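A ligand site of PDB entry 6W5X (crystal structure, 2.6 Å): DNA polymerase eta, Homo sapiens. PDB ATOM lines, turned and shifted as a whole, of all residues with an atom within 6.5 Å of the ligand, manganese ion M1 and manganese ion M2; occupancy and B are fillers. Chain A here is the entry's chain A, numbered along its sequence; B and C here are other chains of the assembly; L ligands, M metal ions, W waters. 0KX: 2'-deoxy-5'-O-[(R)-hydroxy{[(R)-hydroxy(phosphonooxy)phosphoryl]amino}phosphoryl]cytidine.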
ATOM      1  N   ASP A  13      -7.342   9.722 -32.015  1.00  0.00           N
ATOM      2  CA  ASP A  13      -6.321  10.656 -31.574  1.00  0.00           C
ATOM      3  C   ASP A  13      -5.933  11.564 -32.725  1.00  0.00           C
ATOM      4  O   ASP A  13      -5.656  11.100 -33.834  1.00  0.00           O
ATOM      5  CB  ASP A  13      -5.096   9.892 -31.055  1.00  0.00           C
ATOM      6  CG  ASP A  13      -4.010  10.815 -30.589  1.00  0.00           C
ATOM      7  OD1 ASP A  13      -3.293  11.354 -31.451  1.00  0.00           O
ATOM      8  OD2 ASP A  13      -3.864  11.015 -29.361  1.00  0.00           O
ATOM      9  N   MET A  14      -5.917  12.867 -32.483  1.00  0.00           N
ATOM     10  CA  MET A  14      -5.635  13.799 -33.554  1.00  0.00           C
ATOM     11  C   MET A  14      -4.170  13.714 -33.975  1.00  0.00           C
ATOM     12  O   MET A  14      -3.260  13.612 -33.147  1.00  0.00           O
ATOM     13  CB  MET A  14      -5.986  15.229 -33.109  1.00  0.00           C
ATOM     14  CG  MET A  14      -7.379  15.332 -32.455  1.00  0.00           C
ATOM     15  SD  MET A  14      -8.771  14.852 -33.528  1.00  0.00           S
ATOM     16  CE  MET A  14      -8.461  15.944 -34.864  1.00  0.00           C
ATOM     17  N   ASP A  15      -3.946  13.754 -35.287  1.00  0.00           N
ATOM     18  CA  ASP A  15      -2.592  13.814 -35.829  1.00  0.00           C
ATOM     19  C   ASP A  15      -1.980  15.174 -35.549  1.00  0.00           C
ATOM     20  O   ASP A  15      -2.574  16.205 -35.889  1.00  0.00           O
ATOM     21  CB  ASP A  15      -2.606  13.526 -37.330  1.00  0.00           C
ATOM     22  CG  ASP A  15      -3.224  12.169 -37.652  1.00  0.00           C
ATOM     23  OD1 ASP A  15      -3.226  11.294 -36.759  1.00  0.00           O
ATOM     24  OD2 ASP A  15      -3.719  11.978 -38.775  1.00  0.00           O
ATOM     25  N   CYS A  16      -0.793  15.173 -34.947  1.00  0.00           N
ATOM     26  CA  CYS A  16      -0.068  16.377 -34.536  1.00  0.00           C
ATOM     27  C   CYS A  16      -1.018  17.532 -34.220  1.00  0.00           C
ATOM     28  O   CYS A  16      -1.050  18.545 -34.930  1.00  0.00           O
ATOM     29  CB  CYS A  16       0.953  16.758 -35.611  1.00  0.00           C
ATOM     30  SG  CYS A  16       0.338  16.979 -37.312  1.00  0.00           S
ATOM     31  N   PHE A  17      -1.778  17.403 -33.128  1.00  0.00           N
ATOM     32  CA  PHE A  17      -2.963  18.236 -32.925  1.00  0.00           C
ATOM     33  C   PHE A  17      -2.670  19.741 -32.941  1.00  0.00           C
ATOM     34  O   PHE A  17      -3.279  20.502 -33.709  1.00  0.00           O
ATOM     35  CB  PHE A  17      -3.636  17.840 -31.628  1.00  0.00           C
ATOM     36  CG  PHE A  17      -4.889  18.579 -31.374  1.00  0.00           C
ATOM     37  CD1 PHE A  17      -5.822  18.754 -32.379  1.00  0.00           C
ATOM     38  CD2 PHE A  17      -5.141  19.114 -30.126  1.00  0.00           C
ATOM     39  CE1 PHE A  17      -6.996  19.442 -32.154  1.00  0.00           C
ATOM     40  CE2 PHE A  17      -6.324  19.802 -29.874  1.00  0.00           C
ATOM     41  CZ  PHE A  17      -7.259  19.958 -30.902  1.00  0.00           C
ATOM     42  N   PHE A  18      -1.765  20.206 -32.068  1.00  0.00           N
ATOM     43  CA  PHE A  18      -1.536  21.656 -31.987  1.00  0.00           C
ATOM     44  C   PHE A  18      -1.086  22.230 -33.322  1.00  0.00           C
ATOM     45  O   PHE A  18      -1.486  23.334 -33.692  1.00  0.00           O
ATOM     46  CB  PHE A  18      -0.533  22.003 -30.907  1.00  0.00           C
ATOM     47  CG  PHE A  18      -1.035  21.839 -29.492  1.00  0.00           C
ATOM     48  CD1 PHE A  18      -2.180  21.121 -29.201  1.00  0.00           C
ATOM     49  CD2 PHE A  18      -0.326  22.385 -28.440  1.00  0.00           C
ATOM     50  CE1 PHE A  18      -2.610  20.950 -27.893  1.00  0.00           C
ATOM     51  CE2 PHE A  18      -0.754  22.225 -27.132  1.00  0.00           C
ATOM     52  CZ  PHE A  18      -1.899  21.498 -26.863  1.00  0.00           C
ATOM     53  N   VAL A  19      -0.263  21.471 -34.074  1.00  0.00           N
ATOM     54  CA  VAL A  19       0.207  21.920 -35.399  1.00  0.00           C
ATOM     55  C   VAL A  19      -0.962  22.078 -36.361  1.00  0.00           C
ATOM     56  O   VAL A  19      -1.106  23.117 -37.032  1.00  0.00           O
ATOM     57  CB  VAL A  19       1.265  20.953 -35.979  1.00  0.00           C
ATOM     58  CG1 VAL A  19       1.910  21.582 -37.183  1.00  0.00           C
ATOM     59  CG2 VAL A  19       2.359  20.652 -34.969  1.00  0.00           C
ATOM     60  N   GLN A  38       6.579  26.963 -27.148  1.00  0.00           N
ATOM     61  CA  GLN A  38       6.264  27.827 -26.021  1.00  0.00           C
ATOM     62  C   GLN A  38       7.467  28.719 -25.705  1.00  0.00           C
ATOM     63  O   GLN A  38       8.605  28.216 -25.665  1.00  0.00           O
ATOM     64  CB  GLN A  38       5.929  26.996 -24.774  1.00  0.00           C
ATOM     65  CG  GLN A  38       4.476  26.706 -24.587  1.00  0.00           C
ATOM     66  CD  GLN A  38       4.275  25.652 -23.544  1.00  0.00           C
ATOM     67  OE1 GLN A  38       5.223  25.279 -22.873  1.00  0.00           O
ATOM     68  NE2 GLN A  38       3.055  25.155 -23.391  1.00  0.00           N
ATOM     69  N   ILE A  48       6.509  21.640 -28.475  1.00  0.00           N
ATOM     70  CA  ILE A  48       5.472  20.780 -27.918  1.00  0.00           C
ATOM     71  C   ILE A  48       4.661  20.046 -28.970  1.00  0.00           C
ATOM     72  O   ILE A  48       3.875  19.158 -28.610  1.00  0.00           O
ATOM     73  CB  ILE A  48       4.517  21.571 -26.998  1.00  0.00           C
ATOM     74  CG1 ILE A  48       3.611  22.502 -27.796  1.00  0.00           C
ATOM     75  CG2 ILE A  48       5.297  22.361 -25.959  1.00  0.00           C
ATOM     76  CD1 ILE A  48       2.679  23.311 -26.906  1.00  0.00           C
ATOM     77  N   ALA A  49       4.801  20.373 -30.258  1.00  0.00           N
ATOM     78  CA  ALA A  49       4.097  19.611 -31.282  1.00  0.00           C
ATOM     79  C   ALA A  49       4.846  19.793 -32.592  1.00  0.00           C
ATOM     80  O   ALA A  49       5.260  20.899 -32.912  1.00  0.00           O
ATOM     81  CB  ALA A  49       2.627  20.048 -31.408  1.00  0.00           C
ATOM     82  N   VAL A  50       4.978  18.705 -33.341  1.00  0.00           N
ATOM     83  CA  VAL A  50       5.795  18.617 -34.537  1.00  0.00           C
ATOM     84  C   VAL A  50       4.963  18.012 -35.652  1.00  0.00           C
ATOM     85  O   VAL A  50       4.368  16.951 -35.480  1.00  0.00           O
ATOM     86  CB  VAL A  50       7.049  17.742 -34.294  1.00  0.00           C
ATOM     87  CG1 VAL A  50       7.974  17.810 -35.495  1.00  0.00           C
ATOM     88  CG2 VAL A  50       7.751  18.138 -33.038  1.00  0.00           C
ATOM     89  N   TYR A  52       4.335  16.103 -39.319  1.00  0.00           N
ATOM     90  CA  TYR A  52       4.952  14.889 -39.850  1.00  0.00           C
ATOM     91  C   TYR A  52       6.045  15.226 -40.873  1.00  0.00           C
ATOM     92  O   TYR A  52       7.021  14.473 -41.001  1.00  0.00           O
ATOM     93  CB  TYR A  52       3.879  13.950 -40.433  1.00  0.00           C
ATOM     94  CG  TYR A  52       3.193  13.172 -39.350  1.00  0.00           C
ATOM     95  CD1 TYR A  52       2.355  13.804 -38.443  1.00  0.00           C
ATOM     96  CD2 TYR A  52       3.440  11.817 -39.152  1.00  0.00           C
ATOM     97  CE1 TYR A  52       1.759  13.116 -37.408  1.00  0.00           C
ATOM     98  CE2 TYR A  52       2.842  11.118 -38.118  1.00  0.00           C
ATOM     99  CZ  TYR A  52       2.005  11.772 -37.241  1.00  0.00           C
ATOM    100  OH  TYR A  52       1.388  11.106 -36.185  1.00  0.00           O
ATOM    101  N   ARG A  55       9.027  15.821 -38.712  1.00  0.00           N
ATOM    102  CA  ARG A  55       9.510  14.572 -38.132  1.00  0.00           C
ATOM    103  C   ARG A  55      10.384  13.796 -39.115  1.00  0.00           C
ATOM    104  O   ARG A  55      11.223  12.996 -38.688  1.00  0.00           O
ATOM    105  CB  ARG A  55       8.314  13.702 -37.684  1.00  0.00           C
ATOM    106  CG  ARG A  55       7.422  14.335 -36.623  1.00  0.00           C
ATOM    107  CD  ARG A  55       6.322  13.375 -36.106  1.00  0.00           C
ATOM    108  NE  ARG A  55       5.236  14.087 -35.413  1.00  0.00           N
ATOM    109  CZ  ARG A  55       4.189  13.512 -34.841  1.00  0.00           C
ATOM    110  NH1 ARG A  55       4.052  12.195 -34.826  1.00  0.00           N
ATOM    111  NH2 ARG A  55       3.255  14.257 -34.262  1.00  0.00           N
ATOM    112  N   ARG A  61       9.287  16.555 -30.048  1.00  0.00           N
ATOM    113  CA  ARG A  61       8.886  17.276 -28.846  1.00  0.00           C
ATOM    114  C   ARG A  61      10.055  17.401 -27.873  1.00  0.00           C
ATOM    115  O   ARG A  61      11.018  16.626 -27.922  1.00  0.00           O
ATOM    116  CB  ARG A  61       7.712  16.555 -28.194  1.00  0.00           C
ATOM    117  CG  ARG A  61       7.050  17.324 -27.127  1.00  0.00           C
ATOM    118  CD  ARG A  61       5.712  16.725 -26.784  1.00  0.00           C
ATOM    119  NE  ARG A  61       5.591  15.300 -27.105  1.00  0.00           N
ATOM    120  CZ  ARG A  61       4.588  14.771 -27.802  1.00  0.00           C
ATOM    121  NH1 ARG A  61       3.609  15.546 -28.292  1.00  0.00           N
ATOM    122  NH2 ARG A  61       4.555  13.459 -28.005  1.00  0.00           N
ATOM    123  N   LEU A  89      -3.492  28.124 -23.528  1.00  0.00           N
ATOM    124  CA  LEU A  89      -3.853  27.028 -24.396  1.00  0.00           C
ATOM    125  C   LEU A  89      -5.310  27.095 -24.855  1.00  0.00           C
ATOM    126  O   LEU A  89      -5.818  26.139 -25.449  1.00  0.00           O
ATOM    127  CB  LEU A  89      -3.559  25.691 -23.693  1.00  0.00           C
ATOM    128  CG  LEU A  89      -2.136  25.564 -23.140  1.00  0.00           C
ATOM    129  CD1 LEU A  89      -1.967  24.236 -22.426  1.00  0.00           C
ATOM    130  CD2 LEU A  89      -1.096  25.680 -24.242  1.00  0.00           C
ATOM    131  N   SER A 113      -7.530  12.890 -23.231  1.00  0.00           N
ATOM    132  CA  SER A 113      -6.546  13.956 -23.294  1.00  0.00           C
ATOM    133  C   SER A 113      -7.174  15.115 -24.052  1.00  0.00           C
ATOM    134  O   SER A 113      -8.326  15.052 -24.480  1.00  0.00           O
ATOM    135  CB  SER A 113      -5.255  13.485 -23.970  1.00  0.00           C
ATOM    136  OG  SER A 113      -5.298  13.734 -25.375  1.00  0.00           O
ATOM    137  N   ILE A 114      -6.403  16.179 -24.223  1.00  0.00           N
ATOM    138  CA  ILE A 114      -6.913  17.252 -25.062  1.00  0.00           C
ATOM    139  C   ILE A 114      -7.162  16.785 -26.495  1.00  0.00           C
ATOM    140  O   ILE A 114      -8.021  17.368 -27.179  1.00  0.00           O
ATOM    141  CB  ILE A 114      -5.951  18.439 -25.037  1.00  0.00           C
ATOM    142  CG1 ILE A 114      -6.624  19.640 -25.684  1.00  0.00           C
ATOM    143  CG2 ILE A 114      -4.658  18.112 -25.751  1.00  0.00           C
ATOM    144  CD1 ILE A 114      -5.812  20.898 -25.619  1.00  0.00           C
ATOM    145  N   ASP A 115      -6.479  15.750 -26.980  1.00  0.00           N
ATOM    146  CA  ASP A 115      -6.614  15.385 -28.384  1.00  0.00           C
ATOM    147  C   ASP A 115      -7.054  13.934 -28.595  1.00  0.00           C
ATOM    148  O   ASP A 115      -6.944  13.436 -29.725  1.00  0.00           O
ATOM    149  CB  ASP A 115      -5.310  15.626 -29.147  1.00  0.00           C
ATOM    150  CG  ASP A 115      -4.267  14.548 -28.871  1.00  0.00           C
ATOM    151  OD1 ASP A 115      -4.187  14.073 -27.715  1.00  0.00           O
ATOM    152  OD2 ASP A 115      -3.568  14.163 -29.821  1.00  0.00           O
ATOM    153  N   GLU A 116      -7.544  13.250 -27.572  1.00  0.00           N
ATOM    154  CA  GLU A 116      -8.017  11.897 -27.812  1.00  0.00           C
ATOM    155  C   GLU A 116      -9.159  11.541 -26.869  1.00  0.00           C
ATOM    156  O   GLU A 116      -9.215  12.010 -25.733  1.00  0.00           O
ATOM    157  CB  GLU A 116      -6.893  10.875 -27.695  1.00  0.00           C
ATOM    158  CG  GLU A 116      -6.351  10.681 -26.298  1.00  0.00           C
ATOM    159  CD  GLU A 116      -4.863  10.442 -26.342  1.00  0.00           C
ATOM    160  OE1 GLU A 116      -4.144  11.428 -26.608  1.00  0.00           O
ATOM    161  OE2 GLU A 116      -4.424   9.291 -26.169  1.00  0.00           O
ATOM    162  N   SER A 213      -6.169   9.799 -36.420  1.00  0.00           N
ATOM    163  CA  SER A 213      -6.128   8.347 -36.485  1.00  0.00           C
ATOM    164  C   SER A 213      -7.006   7.721 -35.411  1.00  0.00           C
ATOM    165  O   SER A 213      -7.498   8.399 -34.481  1.00  0.00           O
ATOM    166  CB  SER A 213      -4.690   7.844 -36.364  1.00  0.00           C
ATOM    167  OG  SER A 213      -3.835   8.526 -37.257  1.00  0.00           O
ATOM    168  N   LYS A 224      -5.653   1.763 -28.036  1.00  0.00           N
ATOM    169  CA  LYS A 224      -4.603   2.782 -27.958  1.00  0.00           C
ATOM    170  C   LYS A 224      -3.400   2.362 -28.776  1.00  0.00           C
ATOM    171  O   LYS A 224      -2.894   3.125 -29.611  1.00  0.00           O
ATOM    172  CB  LYS A 224      -4.178   3.018 -26.505  1.00  0.00           C
ATOM    173  CG  LYS A 224      -3.354   4.306 -26.246  1.00  0.00           C
ATOM    174  CD  LYS A 224      -1.858   4.107 -26.311  1.00  0.00           C
ATOM    175  CE  LYS A 224      -1.067   5.323 -25.729  1.00  0.00           C
ATOM    176  NZ  LYS A 224      -1.114   6.646 -26.517  1.00  0.00           N
ATOM    177  N   LYS A 231      -0.615   5.754 -37.823  1.00  0.00           N
ATOM    178  CA  LYS A 231      -0.576   7.198 -37.847  1.00  0.00           C
ATOM    179  C   LYS A 231       0.326   7.662 -38.993  1.00  0.00           C
ATOM    180  O   LYS A 231       1.371   7.046 -39.233  1.00  0.00           O
ATOM    181  CB  LYS A 231      -0.048   7.707 -36.494  1.00  0.00           C
ATOM    182  CG  LYS A 231      -0.944   8.704 -35.805  1.00  0.00           C
ATOM    183  CD  LYS A 231      -0.706   8.774 -34.303  1.00  0.00           C
ATOM    184  CE  LYS A 231      -1.968   9.278 -33.571  1.00  0.00           C
ATOM    185  NZ  LYS A 231      -2.336  10.674 -34.008  1.00  0.00           N
ATOM    186  N   PRO A 232      -0.019   8.725 -39.729  1.00  0.00           N
ATOM    187  CA  PRO A 232      -1.207   9.615 -39.649  1.00  0.00           C
ATOM    188  C   PRO A 232      -2.335   9.312 -40.627  1.00  0.00           C
ATOM    189  O   PRO A 232      -2.109   8.690 -41.656  1.00  0.00           O
ATOM    190  CB  PRO A 232      -0.613  10.988 -39.993  1.00  0.00           C
ATOM    191  CG  PRO A 232       0.503  10.681 -40.968  1.00  0.00           C
ATOM    192  CD  PRO A 232       1.059   9.327 -40.541  1.00  0.00           C
ATOM    193  P    DG B   8       0.639   8.945 -23.816  1.00  0.00           P
ATOM    194  OP1  DG B   8       0.088   7.965 -24.799  1.00  0.00           O
ATOM    195  OP2  DG B   8       2.093   9.188 -23.681  1.00  0.00           O
ATOM    196  O5'  DG B   8      -0.048  10.371 -24.060  1.00  0.00           O
ATOM    197  C5'  DG B   8      -1.477  10.529 -24.006  1.00  0.00           C
ATOM    198  C4'  DG B   8      -1.835  11.982 -24.189  1.00  0.00           C
ATOM    199  O4'  DG B   8      -1.281  12.722 -23.072  1.00  0.00           O
ATOM    200  C3'  DG B   8      -1.240  12.591 -25.451  1.00  0.00           C
ATOM    201  O3'  DG B   8      -2.139  13.550 -26.042  1.00  0.00           O
ATOM    202  C2'  DG B   8       0.027  13.261 -24.948  1.00  0.00           C
ATOM    203  C1'  DG B   8      -0.391  13.712 -23.552  1.00  0.00           C
ATOM    204  N9   DG B   8       0.737  13.846 -22.648  1.00  0.00           N
ATOM    205  C8   DG B   8       1.724  12.912 -22.419  1.00  0.00           C
ATOM    206  N7   DG B   8       2.644  13.314 -21.571  1.00  0.00           N
ATOM    207  C5   DG B   8       2.249  14.605 -21.234  1.00  0.00           C
ATOM    208  C6   DG B   8       2.862  15.541 -20.370  1.00  0.00           C
ATOM    209  O6   DG B   8       3.895  15.418 -19.706  1.00  0.00           O
ATOM    210  N1   DG B   8       2.145  16.733 -20.311  1.00  0.00           N
ATOM    211  C2   DG B   8       0.982  16.990 -21.013  1.00  0.00           C
ATOM    212  N2   DG B   8       0.443  18.209 -20.831  1.00  0.00           N
ATOM    213  N3   DG B   8       0.393  16.109 -21.838  1.00  0.00           N
ATOM    214  C4   DG B   8       1.093  14.949 -21.896  1.00  0.00           C
ATOM    215  P    DT C   3      16.003  20.522 -18.345  1.00  0.00           P
ATOM    216  OP1  DT C   3      14.722  20.510 -17.576  1.00  0.00           O
ATOM    217  OP2  DT C   3      17.106  19.649 -17.896  1.00  0.00           O
ATOM    218  O5'  DT C   3      15.704  20.189 -19.883  1.00  0.00           O
ATOM    219  C5'  DT C   3      14.390  19.898 -20.334  1.00  0.00           C
ATOM    220  C4'  DT C   3      13.637  21.174 -20.611  1.00  0.00           C
ATOM    221  O4'  DT C   3      12.886  21.039 -21.859  1.00  0.00           O
ATOM    222  C3'  DT C   3      12.602  21.596 -19.536  1.00  0.00           C
ATOM    223  O3'  DT C   3      12.894  22.911 -18.994  1.00  0.00           O
ATOM    224  C2'  DT C   3      11.281  21.585 -20.289  1.00  0.00           C
ATOM    225  C1'  DT C   3      11.756  21.865 -21.702  1.00  0.00           C
ATOM    226  N1   DT C   3      10.743  21.587 -22.726  1.00  0.00           N
ATOM    227  C2   DT C   3      10.485  22.555 -23.662  1.00  0.00           C
ATOM    228  O2   DT C   3      11.107  23.606 -23.716  1.00  0.00           O
ATOM    229  N3   DT C   3       9.469  22.250 -24.534  1.00  0.00           N
ATOM    230  C4   DT C   3       8.702  21.093 -24.552  1.00  0.00           C
ATOM    231  O4   DT C   3       7.829  20.906 -25.384  1.00  0.00           O
ATOM    232  C5   DT C   3       9.012  20.112 -23.518  1.00  0.00           C
ATOM    233  C7   DT C   3       8.244  18.809 -23.443  1.00  0.00           C
ATOM    234  C6   DT C   3      10.001  20.412 -22.657  1.00  0.00           C
ATOM    235  OP2 7BG C   4      10.900  22.916 -17.344  1.00  0.00           O
ATOM    236  P   7BG C   4      11.644  23.644 -18.404  1.00  0.00           P
ATOM    237  OP1 7BG C   4      12.649  24.663 -18.001  1.00  0.00           O
ATOM    238  O5' 7BG C   4      10.491  24.355 -19.320  1.00  0.00           O
ATOM    239  C5' 7BG C   4       9.152  24.375 -18.818  1.00  0.00           C
ATOM    240  C4' 7BG C   4       8.217  25.291 -19.627  1.00  0.00           C
ATOM    241  O4' 7BG C   4       7.877  24.708 -20.905  1.00  0.00           O
ATOM    242  C3' 7BG C   4       6.871  25.391 -18.862  1.00  0.00           C
ATOM    243  O3' 7BG C   4       6.131  26.588 -19.034  1.00  0.00           O
ATOM    244  C2' 7BG C   4       6.068  24.237 -19.442  1.00  0.00           C
ATOM    245  F1' 7BG C   4       6.172  23.396 -18.546  1.00  0.00           F
ATOM    246  C1' 7BG C   4       6.777  23.733 -20.684  1.00  0.00           C
ATOM    247  N9  7BG C   4       6.872  22.193 -20.574  1.00  0.00           N
ATOM    248  C8  7BG C   4       7.721  21.351 -19.960  1.00  0.00           C
ATOM    249  C4  7BG C   4       5.938  21.424 -21.142  1.00  0.00           C
ATOM    250  N3  7BG C   4       4.866  21.789 -21.870  1.00  0.00           N
ATOM    251  C2  7BG C   4       4.047  20.869 -22.405  1.00  0.00           C
ATOM    252  N2  7BG C   4       2.978  21.233 -23.124  1.00  0.00           N
ATOM    253  N1  7BG C   4       4.321  19.528 -22.174  1.00  0.00           N
ATOM    254  C6  7BG C   4       5.428  19.166 -21.417  1.00  0.00           C
ATOM    255  O6  7BG C   4       5.637  17.969 -21.228  1.00  0.00           O
ATOM    256  C5  7BG C   4       6.220  20.132 -20.908  1.00  0.00           C
ATOM    257  N7  7BG C   4       7.341  20.083 -20.164  1.00  0.00           N
ATOM    258  C10 7BG C   4       8.042  18.844 -19.642  1.00  0.00           C
ATOM    259  C11 7BG C   4       8.939  19.099 -18.398  1.00  0.00           C
ATOM    260  C12 7BG C   4       8.401  19.506 -17.163  1.00  0.00           C
ATOM    261  C13 7BG C   4       9.242  19.726 -16.063  1.00  0.00           C
ATOM    262  C14 7BG C   4      10.614  19.529 -16.185  1.00  0.00           C
ATOM    263  C15 7BG C   4      11.154  19.111 -17.411  1.00  0.00           C
ATOM    264  C16 7BG C   4      10.319  18.900 -18.501  1.00  0.00           C
ATOM    265  P    DC C   5       5.375  26.435 -17.674  1.00  0.00           P
ATOM    266  OP1  DC C   5       5.265  27.903 -17.720  1.00  0.00           O
ATOM    267  OP2  DC C   5       5.708  25.833 -16.378  1.00  0.00           O
ATOM    268  O5'  DC C   5       3.949  25.825 -18.059  1.00  0.00           O
ATOM    269  C5'  DC C   5       3.337  26.174 -19.289  1.00  0.00           C
ATOM    270  C4'  DC C   5       2.125  25.301 -19.555  1.00  0.00           C
ATOM    271  O4'  DC C   5       2.516  23.917 -19.847  1.00  0.00           O
ATOM    272  C3'  DC C   5       1.131  25.206 -18.404  1.00  0.00           C
ATOM    273  O3'  DC C   5      -0.130  25.216 -18.951  1.00  0.00           O
ATOM    274  C2'  DC C   5       1.463  23.847 -17.784  1.00  0.00           C
ATOM    275  C1'  DC C   5       1.744  23.044 -19.032  1.00  0.00           C
ATOM    276  N1   DC C   5       2.513  21.768 -18.794  1.00  0.00           N
ATOM    277  C2   DC C   5       2.174  20.631 -19.525  1.00  0.00           C
ATOM    278  O2   DC C   5       1.257  20.683 -20.354  1.00  0.00           O
ATOM    279  N3   DC C   5       2.870  19.479 -19.318  1.00  0.00           N
ATOM    280  C4   DC C   5       3.851  19.455 -18.425  1.00  0.00           C
ATOM    281  N4   DC C   5       4.498  18.302 -18.253  1.00  0.00           N
ATOM    282  C5   DC C   5       4.224  20.616 -17.674  1.00  0.00           C
ATOM    283  C6   DC C   5       3.524  21.738 -17.882  1.00  0.00           C
HETATM  284  PG  0KX L   1       0.535  12.485 -32.926  1.00  0.00           P
HETATM  285  O1G 0KX L   1       0.187  12.488 -34.350  1.00  0.00           O
HETATM  286  O2G 0KX L   1       1.855  11.931 -32.630  1.00  0.00           O
HETATM  287  O3G 0KX L   1      -0.578  12.087 -32.054  1.00  0.00           O
HETATM  288  PB  0KX L   1       0.253  14.904 -31.392  1.00  0.00           P
HETATM  289  O1B 0KX L   1      -1.223  14.933 -31.432  1.00  0.00           O
HETATM  290  O2B 0KX L   1       0.957  16.194 -31.410  1.00  0.00           O
HETATM  291  O3B 0KX L   1       0.806  14.018 -32.623  1.00  0.00           O
HETATM  292  PA  0KX L   1      -0.107  13.790 -28.858  1.00  0.00           P
HETATM  293  O1A 0KX L   1       0.523  12.894 -27.874  1.00  0.00           O
HETATM  294  O2A 0KX L   1      -1.394  13.068 -29.468  1.00  0.00           O
HETATM  295  N3A 0KX L   1       0.894  14.053 -30.145  1.00  0.00           N
HETATM  296  O5' 0KX L   1      -0.527  15.189 -28.160  1.00  0.00           O
HETATM  297  C5' 0KX L   1      -1.619  16.036 -28.551  1.00  0.00           C
HETATM  298  C4' 0KX L   1      -1.248  17.479 -28.169  1.00  0.00           C
HETATM  299  O4' 0KX L   1      -0.917  17.470 -26.782  1.00  0.00           O
HETATM  300  C3' 0KX L   1       0.082  17.799 -28.770  1.00  0.00           C
HETATM  301  O3' 0KX L   1      -0.089  18.137 -30.144  1.00  0.00           O
HETATM  302  C2' 0KX L   1       0.432  19.010 -27.938  1.00  0.00           C
HETATM  303  C1' 0KX L   1       0.062  18.523 -26.550  1.00  0.00           C
HETATM  304  N1  0KX L   1       1.148  17.859 -25.775  1.00  0.00           N
HETATM  305  C2  0KX L   1       1.885  18.573 -24.912  1.00  0.00           C
HETATM  306  N3  0KX L   1       2.908  17.962 -24.170  1.00  0.00           N
HETATM  307  C4  0KX L   1       3.189  16.588 -24.316  1.00  0.00           C
HETATM  308  C5  0KX L   1       2.430  15.839 -25.218  1.00  0.00           C
HETATM  309  C6  0KX L   1       1.419  16.478 -25.940  1.00  0.00           C
HETATM  310  O2  0KX L   1       1.669  19.785 -24.769  1.00  0.00           O
HETATM  311  N4  0KX L   1       4.145  15.999 -23.609  1.00  0.00           N
HETATM  312 MN    MN M   1      -2.863  12.204 -27.889  1.00  0.00          MN
HETATM  313 MN    MN M   2      -2.293  13.246 -31.251  1.00  0.00          MN
HETATM  314  O   HOH W   1      -0.117   9.967 -30.179  1.00  0.00           O
HETATM  315  O   HOH W   2      -1.504  10.643 -27.824  1.00  0.00           O
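Residues that only touch manganese ion M2: Lys 231 (3.8 Å).
Within 4 Å of manganese ion M2: Asp 13, Met 14, Asp 115 and Lys 231.
The nearest printed residue that does not touch manganese ion M2 is Asp 15 (4.4 Å).
The side-chain carboxylate (OE1) of Glu 116 is bound to manganese ion M1, 2.0 Å away.
Water W2 is bound to manganese ion M1 (2.1 Å).
The side-chain carboxylate (OD2) of Asp 13 binds manganese ion M1.
Manganese ion M1 is bound by the side-chain carboxylate (OD1) of Asp 115, 2.3 Å away.
Manganese ion M1 is bound by O2A of the ligand (2.3 Å).
O3' of DG 8 of chain B binds manganese ion M1, 2.4 Å away.
Slightly farther from manganese ion M1 lies OD2 of Asp 115 (2.8 Å).
Manganese ion M2 is bound by O2A of the ligand, O1B of the ligand, OD2 of Asp 115, OD1 of Asp 13, O of Met 14 and O3G of the ligand.
The backbone carbonyl oxygen (O) of Ser 213 is in hydrogen-bond range of the backbone NH (N) of Asp 13 (2.8 Å).
N2 of DG 8 of chain B sits close to O2 of DC 5 of chain C (2.6 Å).
The side-chain carboxylate (OD1) of Asp 15 lies within salt-bridge range of the side-chain amino group (NZ) of Lys 231 (3.0 Å).
The backbone NH (N) of Glu 116 lies within hydrogen-bond range of the side-chain hydroxyl (OG) of Ser 113 (3.2 Å).
The backbone carbonyl oxygen (O) of Met 14 sits close to the side-chain amino group (NZ) of Lys 231 (3.2 Å).
O4 of DT 3 of chain C lies close to the backbone NH of Ile 48.
The side-chain carboxylate (OD1) of Asp 15 sits at hydrogen-bond distance from the side-chain hydroxyl (OG) of Ser 213 (2.9 Å).
OP1 of DG 8 of chain B is in salt-bridge range of the side-chain amino group of Lys 224 (2.5 Å).
Residues that only touch the ligand: Asp 15, Ile 48, Ala 49, Arg 61 and Ile 114.
Of the 27 residues printed, 16 come within 4 Å of the ligand.
NH1 of Arg 55 lies within salt-bridge range of O2G of the ligand.
N4 of the ligand lies within hydrogen-bond range of O6 of 7BG 4 of chain C, 3.4 Å away.
N of Phe 17 lies within hydrogen-bond range of O2B of the ligand.
The backbone NH (N) of Cys 16 lies within hydrogen-bond range of an oxygen (O1G) of the ligand (2.9 Å).
The side-chain amino group (NZ) of Lys 231 is in salt-bridge range of an oxygen (O1G) of the ligand, 3.1 Å away.
The side-chain hydroxyl of Tyr 52 is in hydrogen-bond range of an oxygen (O1G) of the ligand.
An oxygen (O3') of the ligand sits at hydrogen-bond distance from the backbone NH (N) of Phe 18 (3.3 Å).
Ser 113 touches manganese ion M1 (OG to MN, 3.8 Å).
Within 4 Å of manganese ion M1: Asp 13, Ser 113, Asp 115, Glu 116 and DG 8 of chain B.
The nearest printed residue that does not touch manganese ion M1 is Met 14 (5.5 Å).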
